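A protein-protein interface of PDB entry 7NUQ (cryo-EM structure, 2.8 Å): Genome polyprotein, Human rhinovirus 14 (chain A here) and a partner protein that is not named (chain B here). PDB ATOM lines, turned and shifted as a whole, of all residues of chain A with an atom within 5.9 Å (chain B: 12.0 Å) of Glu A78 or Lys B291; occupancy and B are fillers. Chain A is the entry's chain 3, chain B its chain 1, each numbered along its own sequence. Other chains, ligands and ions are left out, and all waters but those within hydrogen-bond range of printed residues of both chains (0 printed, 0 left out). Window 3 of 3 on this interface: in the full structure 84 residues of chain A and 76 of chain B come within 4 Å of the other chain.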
ATOM      1  N   ASN A  72      26.819 -16.166 -14.155  1.00  0.00           N
ATOM      2  CA  ASN A  72      26.962 -16.210 -12.706  1.00  0.00           C
ATOM      3  C   ASN A  72      28.233 -15.481 -12.297  1.00  0.00           C
ATOM      4  O   ASN A  72      29.282 -15.641 -12.928  1.00  0.00           O
ATOM      5  CB  ASN A  72      26.997 -17.657 -12.202  1.00  0.00           C
ATOM      6  CG  ASN A  72      25.717 -18.410 -12.505  1.00  0.00           C
ATOM      7  OD1 ASN A  72      24.793 -18.442 -11.692  1.00  0.00           O
ATOM      8  ND2 ASN A  72      25.656 -19.023 -13.682  1.00  0.00           N
ATOM      9  N   ARG A  75      32.769 -16.569 -11.041  1.00  0.00           N
ATOM     10  CA  ARG A  75      33.024 -17.853 -11.681  1.00  0.00           C
ATOM     11  C   ARG A  75      34.303 -17.749 -12.500  1.00  0.00           C
ATOM     12  O   ARG A  75      34.374 -16.964 -13.451  1.00  0.00           O
ATOM     13  CB  ARG A  75      31.851 -18.265 -12.570  1.00  0.00           C
ATOM     14  CG  ARG A  75      30.524 -18.391 -11.838  1.00  0.00           C
ATOM     15  CD  ARG A  75      30.584 -19.431 -10.728  1.00  0.00           C
ATOM     16  NE  ARG A  75      29.279 -19.641 -10.106  1.00  0.00           N
ATOM     17  CZ  ARG A  75      28.332 -20.441 -10.590  1.00  0.00           C
ATOM     18  NH1 ARG A  75      28.532 -21.116 -11.715  1.00  0.00           N
ATOM     19  NH2 ARG A  75      27.179 -20.565  -9.948  1.00  0.00           N
ATOM     20  N   GLN A  76      35.306 -18.538 -12.129  1.00  0.00           N
ATOM     21  CA  GLN A  76      36.587 -18.559 -12.817  1.00  0.00           C
ATOM     22  C   GLN A  76      36.739 -19.848 -13.613  1.00  0.00           C
ATOM     23  O   GLN A  76      36.347 -20.928 -13.164  1.00  0.00           O
ATOM     24  CB  GLN A  76      37.740 -18.423 -11.821  1.00  0.00           C
ATOM     25  CG  GLN A  76      37.682 -17.162 -10.976  1.00  0.00           C
ATOM     26  CD  GLN A  76      38.862 -17.035 -10.031  1.00  0.00           C
ATOM     27  OE1 GLN A  76      39.718 -17.915  -9.971  1.00  0.00           O
ATOM     28  NE2 GLN A  76      38.910 -15.934  -9.291  1.00  0.00           N
ATOM     29  N   ASN A  77      37.320 -19.719 -14.803  1.00  0.00           N
ATOM     30  CA  ASN A  77      37.581 -20.841 -15.706  1.00  0.00           C
ATOM     31  C   ASN A  77      36.390 -21.799 -15.754  1.00  0.00           C
ATOM     32  O   ASN A  77      36.486 -22.985 -15.437  1.00  0.00           O
ATOM     33  CB  ASN A  77      38.862 -21.575 -15.308  1.00  0.00           C
ATOM     34  CG  ASN A  77      38.787 -22.180 -13.920  1.00  0.00           C
ATOM     35  OD1 ASN A  77      39.152 -21.543 -12.932  1.00  0.00           O
ATOM     36  ND2 ASN A  77      38.312 -23.419 -13.837  1.00  0.00           N
ATOM     37  N   GLU A  78      35.248 -21.252 -16.166  1.00  0.00           N
ATOM     38  CA  GLU A  78      34.023 -22.023 -16.311  1.00  0.00           C
ATOM     39  C   GLU A  78      33.388 -21.701 -17.655  1.00  0.00           C
ATOM     40  O   GLU A  78      33.587 -20.617 -18.209  1.00  0.00           O
ATOM     41  CB  GLU A  78      33.031 -21.734 -15.174  1.00  0.00           C
ATOM     42  CG  GLU A  78      31.810 -22.641 -15.172  1.00  0.00           C
ATOM     43  CD  GLU A  78      30.882 -22.367 -14.005  1.00  0.00           C
ATOM     44  OE1 GLU A  78      31.119 -21.385 -13.273  1.00  0.00           O
ATOM     45  OE2 GLU A  78      29.915 -23.136 -13.818  1.00  0.00           O
ATOM     46  N   GLN A  79      32.624 -22.657 -18.175  1.00  0.00           N
ATOM     47  CA  GLN A  79      31.970 -22.491 -19.464  1.00  0.00           C
ATOM     48  C   GLN A  79      30.691 -21.676 -19.314  1.00  0.00           C
ATOM     49  O   GLN A  79      29.974 -21.796 -18.317  1.00  0.00           O
ATOM     50  CB  GLN A  79      31.649 -23.853 -20.080  1.00  0.00           C
ATOM     51  CG  GLN A  79      31.046 -23.778 -21.476  1.00  0.00           C
ATOM     52  CD  GLN A  79      30.980 -25.127 -22.178  1.00  0.00           C
ATOM     53  OE1 GLN A  79      30.825 -25.190 -23.397  1.00  0.00           O
ATOM     54  NE2 GLN A  79      31.095 -26.211 -21.415  1.00  0.00           N
ATOM     55  N   VAL A  80      30.412 -20.843 -20.314  1.00  0.00           N
ATOM     56  CA  VAL A  80      29.196 -20.037 -20.333  1.00  0.00           C
ATOM     57  C   VAL A  80      28.116 -20.806 -21.082  1.00  0.00           C
ATOM     58  O   VAL A  80      27.032 -21.061 -20.545  1.00  0.00           O
ATOM     59  CB  VAL A  80      29.444 -18.661 -20.976  1.00  0.00           C
ATOM     60  CG1 VAL A  80      28.164 -17.838 -20.982  1.00  0.00           C
ATOM     61  CG2 VAL A  80      30.555 -17.923 -20.245  1.00  0.00           C
ATOM     62  N   PHE A  81      28.405 -21.178 -22.327  1.00  0.00           N
ATOM     63  CA  PHE A  81      27.477 -21.964 -23.126  1.00  0.00           C
ATOM     64  C   PHE A  81      28.270 -22.770 -24.146  1.00  0.00           C
ATOM     65  O   PHE A  81      29.448 -22.508 -24.399  1.00  0.00           O
ATOM     66  CB  PHE A  81      26.441 -21.075 -23.823  1.00  0.00           C
ATOM     67  CG  PHE A  81      27.019 -20.182 -24.884  1.00  0.00           C
ATOM     68  CD1 PHE A  81      27.478 -18.914 -24.569  1.00  0.00           C
ATOM     69  CD2 PHE A  81      27.100 -20.608 -26.200  1.00  0.00           C
ATOM     70  CE1 PHE A  81      28.009 -18.091 -25.544  1.00  0.00           C
ATOM     71  CE2 PHE A  81      27.630 -19.789 -27.179  1.00  0.00           C
ATOM     72  CZ  PHE A  81      28.085 -18.529 -26.850  1.00  0.00           C
ATOM     73  N   GLY A  82      27.602 -23.761 -24.730  1.00  0.00           N
ATOM     74  CA  GLY A  82      28.210 -24.599 -25.744  1.00  0.00           C
ATOM     75  C   GLY A  82      27.195 -25.086 -26.755  1.00  0.00           C
ATOM     76  O   GLY A  82      26.086 -25.484 -26.384  1.00  0.00           O
ATOM     77  N   THR A  83      27.556 -25.060 -28.035  1.00  0.00           N
ATOM     78  CA  THR A  83      26.623 -25.440 -29.085  1.00  0.00           C
ATOM     79  C   THR A  83      27.402 -25.830 -30.332  1.00  0.00           C
ATOM     80  O   THR A  83      28.472 -25.284 -30.609  1.00  0.00           O
ATOM     81  CB  THR A  83      25.651 -24.299 -29.414  1.00  0.00           C
ATOM     82  OG1 THR A  83      24.645 -24.770 -30.320  1.00  0.00           O
ATOM     83  CG2 THR A  83      26.391 -23.129 -30.047  1.00  0.00           C
ATOM     84  N   ARG A 142      38.788 -24.472 -20.709  1.00  0.00           N
ATOM     85  CA  ARG A 142      39.168 -23.220 -21.355  1.00  0.00           C
ATOM     86  C   ARG A 142      40.509 -23.351 -22.069  1.00  0.00           C
ATOM     87  O   ARG A 142      40.704 -22.767 -23.143  1.00  0.00           O
ATOM     88  CB  ARG A 142      39.220 -22.094 -20.324  1.00  0.00           C
ATOM     89  CG  ARG A 142      39.413 -20.710 -20.928  1.00  0.00           C
ATOM     90  CD  ARG A 142      39.535 -19.642 -19.852  1.00  0.00           C
ATOM     91  NE  ARG A 142      40.739 -19.814 -19.043  1.00  0.00           N
ATOM     92  CZ  ARG A 142      41.095 -19.008 -18.047  1.00  0.00           C
ATOM     93  NH1 ARG A 142      40.340 -17.964 -17.728  1.00  0.00           N
ATOM     94  NH2 ARG A 142      42.208 -19.244 -17.369  1.00  0.00           N
ATOM     95  N   CYS A 189      31.768 -20.548 -25.172  1.00  0.00           N
ATOM     96  CA  CYS A 189      32.215 -19.340 -24.497  1.00  0.00           C
ATOM     97  C   CYS A 189      32.602 -19.685 -23.068  1.00  0.00           C
ATOM     98  O   CYS A 189      31.962 -20.525 -22.428  1.00  0.00           O
ATOM     99  CB  CYS A 189      31.126 -18.260 -24.500  1.00  0.00           C
ATOM    100  SG  CYS A 189      31.593 -16.736 -23.650  1.00  0.00           S
ATOM    101  N   TRP A 190      33.651 -19.035 -22.572  1.00  0.00           N
ATOM    102  CA  TRP A 190      34.193 -19.314 -21.251  1.00  0.00           C
ATOM    103  C   TRP A 190      34.466 -18.005 -20.522  1.00  0.00           C
ATOM    104  O   TRP A 190      34.658 -16.953 -21.139  1.00  0.00           O
ATOM    105  CB  TRP A 190      35.486 -20.139 -21.339  1.00  0.00           C
ATOM    106  CG  TRP A 190      35.380 -21.331 -22.242  1.00  0.00           C
ATOM    107  CD1 TRP A 190      35.378 -21.326 -23.608  1.00  0.00           C
ATOM    108  CD2 TRP A 190      35.268 -22.703 -21.847  1.00  0.00           C
ATOM    109  NE1 TRP A 190      35.266 -22.611 -24.085  1.00  0.00           N
ATOM    110  CE2 TRP A 190      35.198 -23.474 -23.024  1.00  0.00           C
ATOM    111  CE3 TRP A 190      35.218 -23.355 -20.610  1.00  0.00           C
ATOM    112  CZ2 TRP A 190      35.081 -24.861 -23.002  1.00  0.00           C
ATOM    113  CZ3 TRP A 190      35.103 -24.733 -20.591  1.00  0.00           C
ATOM    114  CH2 TRP A 190      35.034 -25.470 -21.778  1.00  0.00           C
ATOM    115  N   TYR A 191      34.479 -18.081 -19.194  1.00  0.00           N
ATOM    116  CA  TYR A 191      34.831 -16.935 -18.366  1.00  0.00           C
ATOM    117  C   TYR A 191      36.341 -16.734 -18.405  1.00  0.00           C
ATOM    118  O   TYR A 191      37.100 -17.611 -17.979  1.00  0.00           O
ATOM    119  CB  TYR A 191      34.353 -17.141 -16.930  1.00  0.00           C
ATOM    120  CG  TYR A 191      32.850 -17.151 -16.776  1.00  0.00           C
ATOM    121  CD1 TYR A 191      32.145 -18.346 -16.717  1.00  0.00           C
ATOM    122  CD2 TYR A 191      32.134 -15.964 -16.686  1.00  0.00           C
ATOM    123  CE1 TYR A 191      30.770 -18.358 -16.574  1.00  0.00           C
ATOM    124  CE2 TYR A 191      30.760 -15.966 -16.544  1.00  0.00           C
ATOM    125  CZ  TYR A 191      30.083 -17.166 -16.489  1.00  0.00           C
ATOM    126  OH  TYR A 191      28.715 -17.175 -16.346  1.00  0.00           O
ATOM    127  N   LYS B 284      14.011 -26.877 -30.636  1.00  0.00           N
ATOM    128  CA  LYS B 284      14.472 -28.223 -30.287  1.00  0.00           C
ATOM    129  C   LYS B 284      15.192 -28.161 -28.947  1.00  0.00           C
ATOM    130  O   LYS B 284      16.317 -27.670 -28.840  1.00  0.00           O
ATOM    131  CB  LYS B 284      15.379 -28.781 -31.377  1.00  0.00           C
ATOM    132  CG  LYS B 284      14.696 -29.766 -32.310  1.00  0.00           C
ATOM    133  CD  LYS B 284      15.663 -30.296 -33.356  1.00  0.00           C
ATOM    134  CE  LYS B 284      15.054 -31.441 -34.150  1.00  0.00           C
ATOM    135  NZ  LYS B 284      13.785 -31.050 -34.824  1.00  0.00           N
ATOM    136  N   LYS B 285      14.535 -28.671 -27.908  1.00  0.00           N
ATOM    137  CA  LYS B 285      15.131 -28.685 -26.579  1.00  0.00           C
ATOM    138  C   LYS B 285      16.452 -29.445 -26.594  1.00  0.00           C
ATOM    139  O   LYS B 285      16.618 -30.423 -27.328  1.00  0.00           O
ATOM    140  CB  LYS B 285      14.168 -29.324 -25.575  1.00  0.00           C
ATOM    141  CG  LYS B 285      14.668 -29.307 -24.137  1.00  0.00           C
ATOM    142  CD  LYS B 285      13.678 -29.972 -23.195  1.00  0.00           C
ATOM    143  CE  LYS B 285      14.186 -29.967 -21.762  1.00  0.00           C
ATOM    144  NZ  LYS B 285      13.254 -30.662 -20.833  1.00  0.00           N
ATOM    145  N   ARG B 286      17.394 -28.984 -25.777  1.00  0.00           N
ATOM    146  CA  ARG B 286      18.696 -29.623 -25.692  1.00  0.00           C
ATOM    147  C   ARG B 286      18.610 -30.930 -24.909  1.00  0.00           C
ATOM    148  O   ARG B 286      17.661 -31.182 -24.161  1.00  0.00           O
ATOM    149  CB  ARG B 286      19.707 -28.695 -25.017  1.00  0.00           C
ATOM    150  CG  ARG B 286      20.151 -27.520 -25.864  1.00  0.00           C
ATOM    151  CD  ARG B 286      20.838 -26.469 -25.006  1.00  0.00           C
ATOM    152  NE  ARG B 286      21.529 -25.462 -25.806  1.00  0.00           N
ATOM    153  CZ  ARG B 286      22.793 -25.555 -26.209  1.00  0.00           C
ATOM    154  NH1 ARG B 286      23.526 -26.616 -25.897  1.00  0.00           N
ATOM    155  NH2 ARG B 286      23.328 -24.582 -26.930  1.00  0.00           N
ATOM    156  N   LYS B 287      19.628 -31.768 -25.095  1.00  0.00           N
ATOM    157  CA  LYS B 287      19.804 -32.980 -24.298  1.00  0.00           C
ATOM    158  C   LYS B 287      20.874 -32.685 -23.254  1.00  0.00           C
ATOM    159  O   LYS B 287      22.068 -32.872 -23.501  1.00  0.00           O
ATOM    160  CB  LYS B 287      20.185 -34.162 -25.183  1.00  0.00           C
ATOM    161  CG  LYS B 287      19.087 -34.607 -26.138  1.00  0.00           C
ATOM    162  CD  LYS B 287      17.900 -35.196 -25.391  1.00  0.00           C
ATOM    163  CE  LYS B 287      16.848 -35.733 -26.347  1.00  0.00           C
ATOM    164  NZ  LYS B 287      15.685 -36.313 -25.622  1.00  0.00           N
ATOM    165  N   GLY B 288      20.444 -32.221 -22.089  1.00  0.00           N
ATOM    166  CA  GLY B 288      21.351 -31.796 -21.042  1.00  0.00           C
ATOM    167  C   GLY B 288      21.275 -30.303 -20.799  1.00  0.00           C
ATOM    168  O   GLY B 288      20.296 -29.625 -21.126  1.00  0.00           O
ATOM    169  N   ASP B 289      22.349 -29.785 -20.211  1.00  0.00           N
ATOM    170  CA  ASP B 289      22.428 -28.372 -19.867  1.00  0.00           C
ATOM    171  C   ASP B 289      22.826 -27.562 -21.102  1.00  0.00           C
ATOM    172  O   ASP B 289      22.988 -28.097 -22.203  1.00  0.00           O
ATOM    173  CB  ASP B 289      23.404 -28.166 -18.713  1.00  0.00           C
ATOM    174  CG  ASP B 289      22.987 -28.908 -17.458  1.00  0.00           C
ATOM    175  OD1 ASP B 289      23.066 -30.153 -17.449  1.00  0.00           O
ATOM    176  OD2 ASP B 289      22.580 -28.244 -16.482  1.00  0.00           O
ATOM    177  N   ILE B 290      22.986 -26.248 -20.925  1.00  0.00           N
ATOM    178  CA  ILE B 290      23.374 -25.374 -22.025  1.00  0.00           C
ATOM    179  C   ILE B 290      24.803 -25.611 -22.485  1.00  0.00           C
ATOM    180  O   ILE B 290      25.173 -25.176 -23.581  1.00  0.00           O
ATOM    181  CB  ILE B 290      23.195 -23.897 -21.616  1.00  0.00           C
ATOM    182  CG1 ILE B 290      23.355 -22.974 -22.826  1.00  0.00           C
ATOM    183  CG2 ILE B 290      24.194 -23.519 -20.529  1.00  0.00           C
ATOM    184  CD1 ILE B 290      23.100 -21.514 -22.514  1.00  0.00           C
ATOM    185  N   LYS B 291      25.613 -26.299 -21.681  1.00  0.00           N
ATOM    186  CA  LYS B 291      27.015 -26.525 -22.001  1.00  0.00           C
ATOM    187  C   LYS B 291      27.237 -27.734 -22.901  1.00  0.00           C
ATOM    188  O   LYS B 291      28.361 -27.936 -23.371  1.00  0.00           O
ATOM    189  CB  LYS B 291      27.822 -26.700 -20.711  1.00  0.00           C
ATOM    190  CG  LYS B 291      27.715 -25.522 -19.755  1.00  0.00           C
ATOM    191  CD  LYS B 291      28.471 -25.782 -18.463  1.00  0.00           C
ATOM    192  CE  LYS B 291      28.302 -24.633 -17.482  1.00  0.00           C
ATOM    193  NZ  LYS B 291      29.024 -24.880 -16.203  1.00  0.00           N
ATOM    194  N   SER B 292      26.206 -28.537 -23.150  1.00  0.00           N
ATOM    195  CA  SER B 292      26.351 -29.705 -24.001  1.00  0.00           C
ATOM    196  C   SER B 292      26.484 -29.292 -25.464  1.00  0.00           C
ATOM    197  O   SER B 292      26.055 -28.210 -25.876  1.00  0.00           O
ATOM    198  CB  SER B 292      25.156 -30.645 -23.831  1.00  0.00           C
ATOM    199  OG  SER B 292      23.945 -29.999 -24.181  1.00  0.00           O
ATOM    200  N   TYR B 293      27.093 -30.175 -26.251  1.00  0.00           N
ATOM    201  CA  TYR B 293      27.292 -29.931 -27.675  1.00  0.00           C
ATOM    202  C   TYR B 293      26.421 -30.862 -28.510  1.00  0.00           C
ATOM    203  O   TYR B 293      25.964 -31.900 -28.033  1.00  0.00           O
ATOM    204  CB  TYR B 293      28.765 -30.115 -28.047  1.00  0.00           C
ATOM    205  CG  TYR B 293      29.697 -29.152 -27.346  1.00  0.00           C
ATOM    206  CD1 TYR B 293      30.306 -29.494 -26.147  1.00  0.00           C
ATOM    207  CD2 TYR B 293      29.966 -27.900 -27.883  1.00  0.00           C
ATOM    208  CE1 TYR B 293      31.159 -28.617 -25.503  1.00  0.00           C
ATOM    209  CE2 TYR B 293      30.816 -27.016 -27.248  1.00  0.00           C
ATOM    210  CZ  TYR B 293      31.410 -27.380 -26.057  1.00  0.00           C
ATOM    211  OH  TYR B 293      32.256 -26.504 -25.419  1.00  0.00           O
ATOM    212  OXT TYR B 293      26.154 -30.596 -29.683  1.00  0.00           O
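Of the 10 printed residues of chain B, 5 touch a printed residue of chain A.
Hydrophobic or aromatic side chains of chain B that line the printed part of chain A: Ile B290 and Tyr B293.
Printed residues of chain A that touch a printed residue of chain B: Glu A78, Gln A79, Val A80, Phe A81, Gly A82 and Thr A83.
Among the printed residues, 12 pairs touch across the chains.
Among the printed residues, Asp or Glu carboxylates within 4 Å of a Lys or Arg side-chain nitrogen of the other chain: Glu A78 with Lys B291.
No residue of chain B comes within 4 Å of Asn A72.
No residue of chain B comes within 4 Å of Asn A77.
Gln A79 touches just these residues of chain B: Lys B291 and Tyr B293.
Gly A82 touches just these residues of chain B: Arg B286, Ile B290, Lys B291, Ser B292 and Tyr B293.
Printed residues of chain B within 4 Å of Thr A83: Arg B286 (3.4 Å) and Tyr B293 (3.7 Å).
Trp A190 touches none of the printed residues of chain B.
No residue of chain B comes within 4 Å of Tyr A191.
Of the printed residues of chain A, Arg B286 touches Gly A82 and Thr A83.
Of the printed residues of chain A, Ile B290 touches Val A80, Phe A81 and Gly A82.
Lys B291 touches just these residues of chain A: Glu A78 (3.1 Å), Gln A79 (3.4 Å) and Gly A82 (3.9 Å).
Printed residues of chain A within 4 Å of Ser B292: Gly A82 (2.8 Å).
Of the printed residues of chain A, Tyr B293 touches Gln A79, Gly A82 and Thr A83.
The nearest residue of chain B that does not touch Glu A78 is Ile B290 (8.8 Å).
Among the printed residues, merely in contact across the chains: Gln A79 with Lys B291, Val A80 with Ile B290, Phe A81 with Ile B290, Gly A82 with Lys B291, Gly A82 with Tyr B293, Thr A83 with Arg B286 and Thr A83 with Tyr B293.
O of Ile B290 is in hydrogen-bond range of NH1 of Arg B286 (3.2 Å).
NH1 of Arg B286 is in hydrogen-bond range of O of Ser B292 (3.0 Å).
O of Asp B289 sits at hydrogen-bond distance from OG of Ser B292, 2.9 Å away.
NH1 of Arg A75 is in salt-bridge range of OE1 of Glu A78, 3.0 Å away.
O of Cys A189 sits at hydrogen-bond distance from N of Val A80, 2.6 Å away.
The backbone NH of Cys A189 sits at hydrogen-bond distance from the backbone carbonyl oxygen of Phe A81.
The guanidinium group (NH1) of Arg B286 is in hydrogen-bond range of the backbone carbonyl oxygen (O) of Gly A82 (2.8 Å).
The backbone carbonyl oxygen (O) of Ile B290 sits at hydrogen-bond distance from the backbone NH (N) of Gly A82 (3.0 Å).
The side-chain carboxylate of Glu A78 is in salt-bridge range of the side-chain amino group of Lys B291.
OH of Tyr B293 sits at hydrogen-bond distance from OE1 of Gln A79.
The backbone carbonyl oxygen of Gly A82 sits close to the backbone carbonyl oxygen of Ser B292.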
